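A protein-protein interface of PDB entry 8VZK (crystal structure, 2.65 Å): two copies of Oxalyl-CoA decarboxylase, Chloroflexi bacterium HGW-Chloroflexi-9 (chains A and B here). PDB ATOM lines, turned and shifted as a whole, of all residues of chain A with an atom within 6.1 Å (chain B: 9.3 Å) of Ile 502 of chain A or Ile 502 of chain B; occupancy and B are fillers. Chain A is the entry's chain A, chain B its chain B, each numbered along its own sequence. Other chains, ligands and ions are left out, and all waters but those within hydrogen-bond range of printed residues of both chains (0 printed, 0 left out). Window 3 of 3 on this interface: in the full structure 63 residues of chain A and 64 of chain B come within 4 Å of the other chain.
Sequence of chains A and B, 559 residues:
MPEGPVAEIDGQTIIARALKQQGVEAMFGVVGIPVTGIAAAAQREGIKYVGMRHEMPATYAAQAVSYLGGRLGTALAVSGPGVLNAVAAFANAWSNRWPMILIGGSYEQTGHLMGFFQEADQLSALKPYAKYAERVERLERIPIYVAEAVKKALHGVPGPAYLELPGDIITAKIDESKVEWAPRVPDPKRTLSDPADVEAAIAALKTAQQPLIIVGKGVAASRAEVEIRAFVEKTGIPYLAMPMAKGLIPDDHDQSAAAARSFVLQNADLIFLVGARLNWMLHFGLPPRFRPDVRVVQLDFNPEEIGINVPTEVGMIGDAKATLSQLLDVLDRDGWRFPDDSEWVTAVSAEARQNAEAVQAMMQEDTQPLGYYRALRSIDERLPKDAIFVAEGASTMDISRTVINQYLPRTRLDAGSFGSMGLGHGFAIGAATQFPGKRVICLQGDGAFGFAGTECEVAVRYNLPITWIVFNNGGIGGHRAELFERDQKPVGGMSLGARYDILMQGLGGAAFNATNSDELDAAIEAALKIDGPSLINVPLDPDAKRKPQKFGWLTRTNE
Among the printed residues, merely in contact across the chains: Ile 502 of chain A with Ile 502 of chain B (3.6 Å), Ile 502 of chain A with Gly 506 of chain B (3.7 Å), Leu 503 of chain A with Leu 503 of chain B (3.7 Å), Leu 503 of chain A with Leu 507 of chain B (3.9 Å), Gly 506 of chain A with Ala 498 of chain B (3.7 Å), Gly 506 of chain A with Ile 502 of chain B (3.7 Å) and Leu 507 of chain A with Leu 503 of chain B (3.8 Å).
Of the 11 printed residues of chain A, 5 touch a printed residue of chain B. Printed residues of chain A that touch a printed residue of chain B: Arg 499, Ile 502, Leu 503, Gly 506 and Leu 507. Hydrophobic or aromatic side chains of chain A that line the printed part of chain B: Ile 502, Leu 503 and Leu 507. Of the 23 printed residues of chain B, 6 touch a printed residue of chain A. Hydrophobic or aromatic side chains of chain B within 4 Å of the printed part of chain A: Ile 502, Leu 503 and Leu 507. Among the printed residues, no Asp or Glu carboxylate lies within 4 Å of a Lys or Arg side-chain nitrogen of the other chain.
The side-chain carboxylate (OD2) of Asp 501 of chain A lies within salt-bridge range of the guanidinium group (NH2) of Arg 499 of chain A (2.8 Å). NH2 of Arg 499 of chain B lies within salt-bridge range of OD2 of Asp 501 of chain B. The guanidinium group of Arg 499 of chain B lies within hydrogen-bond range of the side-chain amide oxygen of Asn 513 of chain B (2.7 Å).
The backbone carbonyl oxygen of Gly 506 of chain B sits at hydrogen-bond distance from the backbone NH of Arg 499 of chain A (2.8 Å). O of Gly 506 of chain A lies within hydrogen-bond range of N of Arg 499 of chain B (2.7 Å).
Arg 499 of chain A touches Gly 506 of chain B, and with the chains exchanged Gly 506 of chain A touches Arg 499 of chain B. Ile 502 of chain A touches Gly 506 of chain B, and with the chains exchanged Gly 506 of chain A touches Ile 502 of chain B. Leu 503 of chain B touches its own counterpart, Leu 503 of chain A. Leu 503 of chain A touches Leu 507 of chain B, and with the chains exchanged Leu 507 of chain A touches Leu 503 of chain B.
Of the printed residues of chain B, Ile 502 of chain A touches Ile 502 (3.6 Å) and Gly 506 (3.7 Å). Gly 506 of chain A touches just these residues of chain B: Ala 498, Arg 499 and Ile 502. Printed residues of chain B within 4 Å of Leu 507 of chain A: Leu 503. Of the printed residues of chain A, Ala 498 of chain B touches Gly 506 (3.7 Å). Of the printed residues of chain A, Arg 499 of chain B touches Gly 506. Ile 502 of chain B touches just these residues of chain A: Ile 502 and Gly 506. Of the printed residues of chain A, Leu 507 of chain B touches Leu 503 (3.9 Å).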
ATOM      1  N   ARG A 499     -15.748 -21.126  -6.162  1.00  0.00           N
ATOM      2  CA  ARG A 499     -15.731 -19.902  -6.960  1.00  0.00           C
ATOM      3  C   ARG A 499     -16.484 -20.178  -8.260  1.00  0.00           C
ATOM      4  O   ARG A 499     -15.890 -20.554  -9.271  1.00  0.00           O
ATOM      5  CB  ARG A 499     -14.299 -19.446  -7.228  1.00  0.00           C
ATOM      6  CG  ARG A 499     -13.574 -18.897  -6.011  1.00  0.00           C
ATOM      7  CD  ARG A 499     -14.076 -17.508  -5.658  1.00  0.00           C
ATOM      8  NE  ARG A 499     -13.878 -16.571  -6.757  1.00  0.00           N
ATOM      9  CZ  ARG A 499     -12.774 -15.862  -6.946  1.00  0.00           C
ATOM     10  NH1 ARG A 499     -11.749 -15.947  -6.115  1.00  0.00           N
ATOM     11  NH2 ARG A 499     -12.696 -15.051  -7.997  1.00  0.00           N
ATOM     12  N   TYR A 500     -17.805 -19.979  -8.227  1.00  0.00           N
ATOM     13  CA  TYR A 500     -18.617 -20.216  -9.414  1.00  0.00           C
ATOM     14  C   TYR A 500     -18.361 -19.185 -10.505  1.00  0.00           C
ATOM     15  O   TYR A 500     -18.721 -19.424 -11.663  1.00  0.00           O
ATOM     16  CB  TYR A 500     -20.101 -20.242  -9.041  1.00  0.00           C
ATOM     17  CG  TYR A 500     -20.443 -21.297  -8.012  1.00  0.00           C
ATOM     18  CD1 TYR A 500     -20.460 -22.645  -8.350  1.00  0.00           C
ATOM     19  CD2 TYR A 500     -20.745 -20.946  -6.703  1.00  0.00           C
ATOM     20  CE1 TYR A 500     -20.768 -23.614  -7.411  1.00  0.00           C
ATOM     21  CE2 TYR A 500     -21.055 -21.908  -5.759  1.00  0.00           C
ATOM     22  CZ  TYR A 500     -21.065 -23.239  -6.118  1.00  0.00           C
ATOM     23  OH  TYR A 500     -21.373 -24.198  -5.180  1.00  0.00           O
ATOM     24  N   ASP A 501     -17.749 -18.047 -10.166  1.00  0.00           N
ATOM     25  CA  ASP A 501     -17.347 -17.098 -11.198  1.00  0.00           C
ATOM     26  C   ASP A 501     -16.187 -17.647 -12.021  1.00  0.00           C
ATOM     27  O   ASP A 501     -16.126 -17.436 -13.237  1.00  0.00           O
ATOM     28  CB  ASP A 501     -16.974 -15.758 -10.566  1.00  0.00           C
ATOM     29  CG  ASP A 501     -15.853 -15.883  -9.555  1.00  0.00           C
ATOM     30  OD1 ASP A 501     -15.776 -16.929  -8.878  1.00  0.00           O
ATOM     31  OD2 ASP A 501     -15.045 -14.938  -9.440  1.00  0.00           O
ATOM     32  N   ILE A 502     -15.259 -18.355 -11.373  1.00  0.00           N
ATOM     33  CA  ILE A 502     -14.190 -19.020 -12.108  1.00  0.00           C
ATOM     34  C   ILE A 502     -14.751 -20.166 -12.940  1.00  0.00           C
ATOM     35  O   ILE A 502     -14.228 -20.477 -14.017  1.00  0.00           O
ATOM     36  CB  ILE A 502     -13.095 -19.496 -11.135  1.00  0.00           C
ATOM     37  CG1 ILE A 502     -12.586 -18.320 -10.298  1.00  0.00           C
ATOM     38  CG2 ILE A 502     -11.940 -20.136 -11.887  1.00  0.00           C
ATOM     39  CD1 ILE A 502     -11.436 -18.674  -9.383  1.00  0.00           C
ATOM     40  N   LEU A 503     -15.823 -20.807 -12.468  1.00  0.00           N
ATOM     41  CA  LEU A 503     -16.523 -21.787 -13.292  1.00  0.00           C
ATOM     42  C   LEU A 503     -17.059 -21.137 -14.561  1.00  0.00           C
ATOM     43  O   LEU A 503     -16.893 -21.668 -15.665  1.00  0.00           O
ATOM     44  CB  LEU A 503     -17.652 -22.434 -12.486  1.00  0.00           C
ATOM     45  CG  LEU A 503     -18.596 -23.424 -13.179  1.00  0.00           C
ATOM     46  CD1 LEU A 503     -18.979 -24.540 -12.220  1.00  0.00           C
ATOM     47  CD2 LEU A 503     -19.848 -22.728 -13.699  1.00  0.00           C
ATOM     48  N   MET A 504     -17.704 -19.977 -14.419  1.00  0.00           N
ATOM     49  CA  MET A 504     -18.193 -19.248 -15.586  1.00  0.00           C
ATOM     50  C   MET A 504     -17.040 -18.753 -16.448  1.00  0.00           C
ATOM     51  O   MET A 504     -17.132 -18.764 -17.682  1.00  0.00           O
ATOM     52  CB  MET A 504     -19.071 -18.082 -15.139  1.00  0.00           C
ATOM     53  CG  MET A 504     -19.463 -17.126 -16.253  1.00  0.00           C
ATOM     54  SD  MET A 504     -20.408 -17.926 -17.561  1.00  0.00           S
ATOM     55  CE  MET A 504     -21.923 -16.971 -17.512  1.00  0.00           C
ATOM     56  N   GLN A 505     -15.948 -18.315 -15.816  1.00  0.00           N
ATOM     57  CA  GLN A 505     -14.786 -17.855 -16.569  1.00  0.00           C
ATOM     58  C   GLN A 505     -14.208 -18.974 -17.428  1.00  0.00           C
ATOM     59  O   GLN A 505     -13.854 -18.753 -18.592  1.00  0.00           O
ATOM     60  CB  GLN A 505     -13.726 -17.309 -15.614  1.00  0.00           C
ATOM     61  CG  GLN A 505     -12.436 -16.886 -16.298  1.00  0.00           C
ATOM     62  CD  GLN A 505     -11.421 -16.313 -15.329  1.00  0.00           C
ATOM     63  OE1 GLN A 505     -11.358 -15.101 -15.124  1.00  0.00           O
ATOM     64  NE2 GLN A 505     -10.619 -17.185 -14.728  1.00  0.00           N
ATOM     65  N   GLY A 506     -14.107 -20.182 -16.870  1.00  0.00           N
ATOM     66  CA  GLY A 506     -13.608 -21.305 -17.644  1.00  0.00           C
ATOM     67  C   GLY A 506     -14.514 -21.687 -18.795  1.00  0.00           C
ATOM     68  O   GLY A 506     -14.047 -22.224 -19.804  1.00  0.00           O
ATOM     69  N   LEU A 507     -15.814 -21.416 -18.669  1.00  0.00           N
ATOM     70  CA  LEU A 507     -16.762 -21.707 -19.736  1.00  0.00           C
ATOM     71  C   LEU A 507     -16.796 -20.628 -20.811  1.00  0.00           C
ATOM     72  O   LEU A 507     -17.450 -20.825 -21.841  1.00  0.00           O
ATOM     73  CB  LEU A 507     -18.164 -21.905 -19.153  1.00  0.00           C
ATOM     74  CG  LEU A 507     -18.336 -23.098 -18.208  1.00  0.00           C
ATOM     75  CD1 LEU A 507     -19.724 -23.103 -17.585  1.00  0.00           C
ATOM     76  CD2 LEU A 507     -18.068 -24.408 -18.933  1.00  0.00           C
ATOM     77  N   ALA A 511     -16.509 -12.873 -15.215  1.00  0.00           N
ATOM     78  CA  ALA A 511     -16.461 -13.372 -13.848  1.00  0.00           C
ATOM     79  C   ALA A 511     -16.321 -12.219 -12.866  1.00  0.00           C
ATOM     80  O   ALA A 511     -15.595 -11.254 -13.123  1.00  0.00           O
ATOM     81  CB  ALA A 511     -15.302 -14.356 -13.657  1.00  0.00           C
ATOM     82  N   ASN A 537     -20.094 -14.001  -8.437  1.00  0.00           N
ATOM     83  CA  ASN A 537     -20.006 -14.857  -7.263  1.00  0.00           C
ATOM     84  C   ASN A 537     -20.104 -13.991  -6.013  1.00  0.00           C
ATOM     85  O   ASN A 537     -19.340 -13.031  -5.853  1.00  0.00           O
ATOM     86  CB  ASN A 537     -18.702 -15.656  -7.282  1.00  0.00           C
ATOM     87  CG  ASN A 537     -18.691 -16.789  -6.268  1.00  0.00           C
ATOM     88  OD1 ASN A 537     -18.787 -17.962  -6.632  1.00  0.00           O
ATOM     89  ND2 ASN A 537     -18.556 -16.445  -4.994  1.00  0.00           N
ATOM     90  N   PHE B 449     -19.806 -34.440 -20.431  1.00  0.00           N
ATOM     91  CA  PHE B 449     -19.427 -33.776 -19.188  1.00  0.00           C
ATOM     92  C   PHE B 449     -20.480 -32.762 -18.751  1.00  0.00           C
ATOM     93  O   PHE B 449     -20.715 -32.585 -17.549  1.00  0.00           O
ATOM     94  CB  PHE B 449     -18.065 -33.099 -19.358  1.00  0.00           C
ATOM     95  CG  PHE B 449     -17.569 -32.397 -18.123  1.00  0.00           C
ATOM     96  CD1 PHE B 449     -16.898 -33.096 -17.133  1.00  0.00           C
ATOM     97  CD2 PHE B 449     -17.759 -31.034 -17.960  1.00  0.00           C
ATOM     98  CE1 PHE B 449     -16.438 -32.452 -15.999  1.00  0.00           C
ATOM     99  CE2 PHE B 449     -17.302 -30.384 -16.829  1.00  0.00           C
ATOM    100  CZ  PHE B 449     -16.640 -31.094 -15.848  1.00  0.00           C
ATOM    101  N   VAL B 470     -11.434 -34.760 -19.957  1.00  0.00           N
ATOM    102  CA  VAL B 470     -12.460 -34.279 -20.874  1.00  0.00           C
ATOM    103  C   VAL B 470     -11.837 -34.093 -22.251  1.00  0.00           C
ATOM    104  O   VAL B 470     -10.747 -33.520 -22.374  1.00  0.00           O
ATOM    105  CB  VAL B 470     -13.089 -32.969 -20.372  1.00  0.00           C
ATOM    106  CG1 VAL B 470     -14.236 -32.549 -21.276  1.00  0.00           C
ATOM    107  CG2 VAL B 470     -13.561 -33.124 -18.933  1.00  0.00           C
ATOM    108  N   GLY B 497     -13.482 -23.550 -27.205  1.00  0.00           N
ATOM    109  CA  GLY B 497     -12.551 -22.921 -26.296  1.00  0.00           C
ATOM    110  C   GLY B 497     -12.900 -23.054 -24.832  1.00  0.00           C
ATOM    111  O   GLY B 497     -12.290 -22.376 -23.999  1.00  0.00           O
ATOM    112  N   ALA B 498     -13.862 -23.906 -24.490  1.00  0.00           N
ATOM    113  CA  ALA B 498     -14.252 -24.073 -23.098  1.00  0.00           C
ATOM    114  C   ALA B 498     -13.134 -24.738 -22.306  1.00  0.00           C
ATOM    115  O   ALA B 498     -12.526 -25.715 -22.754  1.00  0.00           O
ATOM    116  CB  ALA B 498     -15.533 -24.899 -23.000  1.00  0.00           C
ATOM    117  N   ARG B 499     -12.862 -24.197 -21.124  1.00  0.00           N
ATOM    118  CA  ARG B 499     -11.806 -24.682 -20.238  1.00  0.00           C
ATOM    119  C   ARG B 499     -12.468 -25.370 -19.047  1.00  0.00           C
ATOM    120  O   ARG B 499     -12.711 -24.749 -18.012  1.00  0.00           O
ATOM    121  CB  ARG B 499     -10.903 -23.539 -19.789  1.00  0.00           C
ATOM    122  CG  ARG B 499     -10.081 -22.912 -20.901  1.00  0.00           C
ATOM    123  CD  ARG B 499      -8.978 -23.848 -21.361  1.00  0.00           C
ATOM    124  NE  ARG B 499      -8.128 -24.267 -20.251  1.00  0.00           N
ATOM    125  CZ  ARG B 499      -7.119 -23.554 -19.771  1.00  0.00           C
ATOM    126  NH1 ARG B 499      -6.800 -22.375 -20.279  1.00  0.00           N
ATOM    127  NH2 ARG B 499      -6.409 -24.037 -18.754  1.00  0.00           N
ATOM    128  N   TYR B 500     -12.759 -26.664 -19.200  1.00  0.00           N
ATOM    129  CA  TYR B 500     -13.365 -27.416 -18.109  1.00  0.00           C
ATOM    130  C   TYR B 500     -12.394 -27.645 -16.958  1.00  0.00           C
ATOM    131  O   TYR B 500     -12.834 -27.952 -15.845  1.00  0.00           O
ATOM    132  CB  TYR B 500     -13.902 -28.753 -18.624  1.00  0.00           C
ATOM    133  CG  TYR B 500     -14.912 -28.605 -19.741  1.00  0.00           C
ATOM    134  CD1 TYR B 500     -16.197 -28.145 -19.486  1.00  0.00           C
ATOM    135  CD2 TYR B 500     -14.578 -28.923 -21.051  1.00  0.00           C
ATOM    136  CE1 TYR B 500     -17.122 -28.005 -20.506  1.00  0.00           C
ATOM    137  CE2 TYR B 500     -15.495 -28.788 -22.075  1.00  0.00           C
ATOM    138  CZ  TYR B 500     -16.764 -28.329 -21.798  1.00  0.00           C
ATOM    139  OH  TYR B 500     -17.678 -28.195 -22.819  1.00  0.00           O
ATOM    140  N   ASP B 501     -11.089 -27.502 -17.198  1.00  0.00           N
ATOM    141  CA  ASP B 501     -10.130 -27.567 -16.100  1.00  0.00           C
ATOM    142  C   ASP B 501     -10.242 -26.341 -15.203  1.00  0.00           C
ATOM    143  O   ASP B 501     -10.137 -26.450 -13.977  1.00  0.00           O
ATOM    144  CB  ASP B 501      -8.711 -27.707 -16.650  1.00  0.00           C
ATOM    145  CG  ASP B 501      -8.372 -26.636 -17.668  1.00  0.00           C
ATOM    146  OD1 ASP B 501      -9.298 -25.927 -18.114  1.00  0.00           O
ATOM    147  OD2 ASP B 501      -7.181 -26.502 -18.019  1.00  0.00           O
ATOM    148  N   ILE B 502     -10.456 -25.164 -15.798  1.00  0.00           N
ATOM    149  CA  ILE B 502     -10.693 -23.965 -15.001  1.00  0.00           C
ATOM    150  C   ILE B 502     -12.016 -24.078 -14.256  1.00  0.00           C
ATOM    151  O   ILE B 502     -12.172 -23.527 -13.160  1.00  0.00           O
ATOM    152  CB  ILE B 502     -10.640 -22.714 -15.898  1.00  0.00           C
ATOM    153  CG1 ILE B 502      -9.294 -22.639 -16.621  1.00  0.00           C
ATOM    154  CG2 ILE B 502     -10.858 -21.450 -15.082  1.00  0.00           C
ATOM    155  CD1 ILE B 502      -9.111 -21.382 -17.443  1.00  0.00           C
ATOM    156  N   LEU B 503     -12.988 -24.796 -14.828  1.00  0.00           N
ATOM    157  CA  LEU B 503     -14.216 -25.089 -14.098  1.00  0.00           C
ATOM    158  C   LEU B 503     -13.923 -25.920 -12.855  1.00  0.00           C
ATOM    159  O   LEU B 503     -14.485 -25.668 -11.782  1.00  0.00           O
ATOM    160  CB  LEU B 503     -15.209 -25.808 -15.015  1.00  0.00           C
ATOM    161  CG  LEU B 503     -16.576 -26.234 -14.471  1.00  0.00           C
ATOM    162  CD1 LEU B 503     -17.637 -26.093 -15.551  1.00  0.00           C
ATOM    163  CD2 LEU B 503     -16.547 -27.666 -13.952  1.00  0.00           C
ATOM    164  N   MET B 504     -13.039 -26.912 -12.978  1.00  0.00           N
ATOM    165  CA  MET B 504     -12.652 -27.708 -11.818  1.00  0.00           C
ATOM    166  C   MET B 504     -11.842 -26.880 -10.827  1.00  0.00           C
ATOM    167  O   MET B 504     -12.021 -27.012  -9.610  1.00  0.00           O
ATOM    168  CB  MET B 504     -11.862 -28.938 -12.265  1.00  0.00           C
ATOM    169  CG  MET B 504     -11.182 -29.683 -11.127  1.00  0.00           C
ATOM    170  SD  MET B 504     -12.349 -30.386  -9.945  1.00  0.00           S
ATOM    171  CE  MET B 504     -12.518 -32.045 -10.593  1.00  0.00           C
ATOM    172  N   GLN B 505     -10.947 -26.024 -11.329  1.00  0.00           N
ATOM    173  CA  GLN B 505     -10.168 -25.162 -10.445  1.00  0.00           C
ATOM    174  C   GLN B 505     -11.070 -24.221  -9.659  1.00  0.00           C
ATOM    175  O   GLN B 505     -10.806 -23.927  -8.487  1.00  0.00           O
ATOM    176  CB  GLN B 505      -9.142 -24.365 -11.249  1.00  0.00           C
ATOM    177  CG  GLN B 505      -8.275 -23.455 -10.394  1.00  0.00           C
ATOM    178  CD  GLN B 505      -7.737 -22.265 -11.161  1.00  0.00           C
ATOM    179  OE1 GLN B 505      -7.680 -22.276 -12.390  1.00  0.00           O
ATOM    180  NE2 GLN B 505      -7.347 -21.223 -10.435  1.00  0.00           N
ATOM    181  N   GLY B 506     -12.140 -23.731 -10.290  1.00  0.00           N
ATOM    182  CA  GLY B 506     -13.083 -22.884  -9.583  1.00  0.00           C
ATOM    183  C   GLY B 506     -13.832 -23.616  -8.490  1.00  0.00           C
ATOM    184  O   GLY B 506     -14.234 -23.007  -7.493  1.00  0.00           O
ATOM    185  N   LEU B 507     -14.030 -24.923  -8.652  1.00  0.00           N
ATOM    186  CA  LEU B 507     -14.703 -25.722  -7.638  1.00  0.00           C
ATOM    187  C   LEU B 507     -13.762 -26.211  -6.546  1.00  0.00           C
ATOM    188  O   LEU B 507     -14.235 -26.645  -5.490  1.00  0.00           O
ATOM    189  CB  LEU B 507     -15.402 -26.922  -8.289  1.00  0.00           C
ATOM    190  CG  LEU B 507     -16.482 -26.588  -9.322  1.00  0.00           C
ATOM    191  CD1 LEU B 507     -17.134 -27.854  -9.861  1.00  0.00           C
ATOM    192  CD2 LEU B 507     -17.527 -25.654  -8.729  1.00  0.00           C
ATOM    193  N   GLY B 508     -12.451 -26.153  -6.772  1.00  0.00           N
ATOM    194  CA  GLY B 508     -11.491 -26.534  -5.753  1.00  0.00           C
ATOM    195  C   GLY B 508     -10.674 -27.765  -6.089  1.00  0.00           C
ATOM    196  O   GLY B 508     -10.205 -28.466  -5.187  1.00  0.00           O
ATOM    197  N   GLY B 509     -10.489 -28.038  -7.377  1.00  0.00           N
ATOM    198  CA  GLY B 509      -9.714 -29.189  -7.794  1.00  0.00           C
ATOM    199  C   GLY B 509      -8.524 -28.833  -8.661  1.00  0.00           C
ATOM    200  O   GLY B 509      -8.446 -27.722  -9.192  1.00  0.00           O
ATOM    201  N   ALA B 510      -7.589 -29.768  -8.811  1.00  0.00           N
ATOM    202  CA  ALA B 510      -6.421 -29.530  -9.648  1.00  0.00           C
ATOM    203  C   ALA B 510      -6.826 -29.456 -11.115  1.00  0.00           C
ATOM    204  O   ALA B 510      -7.657 -30.234 -11.590  1.00  0.00           O
ATOM    205  CB  ALA B 510      -5.384 -30.633  -9.441  1.00  0.00           C
ATOM    206  N   ALA B 511      -6.229 -28.510 -11.836  1.00  0.00           N
ATOM    207  CA  ALA B 511      -6.555 -28.255 -13.231  1.00  0.00           C
ATOM    208  C   ALA B 511      -5.360 -28.576 -14.117  1.00  0.00           C
ATOM    209  O   ALA B 511      -4.208 -28.351 -13.731  1.00  0.00           O
ATOM    210  CB  ALA B 511      -6.979 -26.799 -13.439  1.00  0.00           C
ATOM    211  N   PHE B 512      -5.642 -29.103 -15.306  1.00  0.00           N
ATOM    212  CA  PHE B 512      -4.611 -29.430 -16.280  1.00  0.00           C
ATOM    213  C   PHE B 512      -5.159 -29.186 -17.677  1.00  0.00           C
ATOM    214  O   PHE B 512      -6.318 -29.499 -17.960  1.00  0.00           O
ATOM    215  CB  PHE B 512      -4.146 -30.886 -16.152  1.00  0.00           C
ATOM    216  CG  PHE B 512      -3.466 -31.198 -14.850  1.00  0.00           C
ATOM    217  CD1 PHE B 512      -2.101 -31.019 -14.709  1.00  0.00           C
ATOM    218  CD2 PHE B 512      -4.189 -31.679 -13.772  1.00  0.00           C
ATOM    219  CE1 PHE B 512      -1.471 -31.308 -13.515  1.00  0.00           C
ATOM    220  CE2 PHE B 512      -3.564 -31.970 -12.574  1.00  0.00           C
ATOM    221  CZ  PHE B 512      -2.203 -31.784 -12.446  1.00  0.00           C
ATOM    222  N   ASN B 513      -4.319 -28.628 -18.545  1.00  0.00           N
ATOM    223  CA  ASN B 513      -4.647 -28.427 -19.951  1.00  0.00           C
ATOM    224  C   ASN B 513      -3.574 -29.107 -20.788  1.00  0.00           C
ATOM    225  O   ASN B 513      -2.406 -28.708 -20.745  1.00  0.00           O
ATOM    226  CB  ASN B 513      -4.744 -26.937 -20.290  1.00  0.00           C
ATOM    227  CG  ASN B 513      -5.525 -26.676 -21.570  1.00  0.00           C
ATOM    228  OD1 ASN B 513      -6.500 -25.928 -21.569  1.00  0.00           O
ATOM    229  ND2 ASN B 513      -5.096 -27.291 -22.666  1.00  0.00           N
ATOM    230  N   SER B 534      -9.130 -34.045  -9.555  1.00  0.00           N
ATOM    231  CA  SER B 534      -8.433 -33.294 -10.589  1.00  0.00           C
ATOM    232  C   SER B 534      -9.169 -33.474 -11.908  1.00  0.00           C
ATOM    233  O   SER B 534      -9.929 -34.429 -12.091  1.00  0.00           O
ATOM    234  CB  SER B 534      -6.974 -33.744 -10.720  1.00  0.00           C
ATOM    235  OG  SER B 534      -6.890 -35.151 -10.865  1.00  0.00           O
ATOM    236  N   LEU B 535      -8.934 -32.538 -12.826  1.00  0.00           N
ATOM    237  CA  LEU B 535      -9.517 -32.596 -14.161  1.00  0.00           C
ATOM    238  C   LEU B 535      -8.456 -32.218 -15.181  1.00  0.00           C
ATOM    239  O   LEU B 535      -7.772 -31.203 -15.022  1.00  0.00           O
ATOM    240  CB  LEU B 535     -10.731 -31.664 -14.282  1.00  0.00           C
ATOM    241  CG  LEU B 535     -11.653 -31.823 -15.498  1.00  0.00           C
ATOM    242  CD1 LEU B 535     -13.056 -31.364 -15.149  1.00  0.00           C
ATOM    243  CD2 LEU B 535     -11.140 -31.059 -16.713  1.00  0.00           C
ATOM    244  N   ILE B 536      -8.326 -33.032 -16.224  1.00  0.00           N
ATOM    245  CA  ILE B 536      -7.387 -32.791 -17.313  1.00  0.00           C
ATOM    246  C   ILE B 536      -8.201 -32.418 -18.543  1.00  0.00           C
ATOM    247  O   ILE B 536      -8.939 -33.250 -19.086  1.00  0.00           O
ATOM    248  CB  ILE B 536      -6.498 -34.013 -17.584  1.00  0.00           C
ATOM    249  CG1 ILE B 536      -5.720 -34.400 -16.325  1.00  0.00           C
ATOM    250  CG2 ILE B 536      -5.546 -33.734 -18.736  1.00  0.00           C
ATOM    251  CD1 ILE B 536      -4.834 -35.613 -16.506  1.00  0.00           C
ATOM    252  N   ASN B 537      -8.077 -31.168 -18.982  1.00  0.00           N
ATOM    253  CA  ASN B 537      -8.779 -30.684 -20.166  1.00  0.00           C
ATOM    254  C   ASN B 537      -7.900 -30.942 -21.384  1.00  0.00           C
ATOM    255  O   ASN B 537      -6.816 -30.363 -21.510  1.00  0.00           O
ATOM    256  CB  ASN B 537      -9.114 -29.201 -20.029  1.00  0.00           C
ATOM    257  CG  ASN B 537     -10.028 -28.704 -21.134  1.00  0.00           C
ATOM    258  OD1 ASN B 537     -11.248 -28.657 -20.973  1.00  0.00           O
ATOM    259  ND2 ASN B 537      -9.441 -28.328 -22.265  1.00  0.00           N
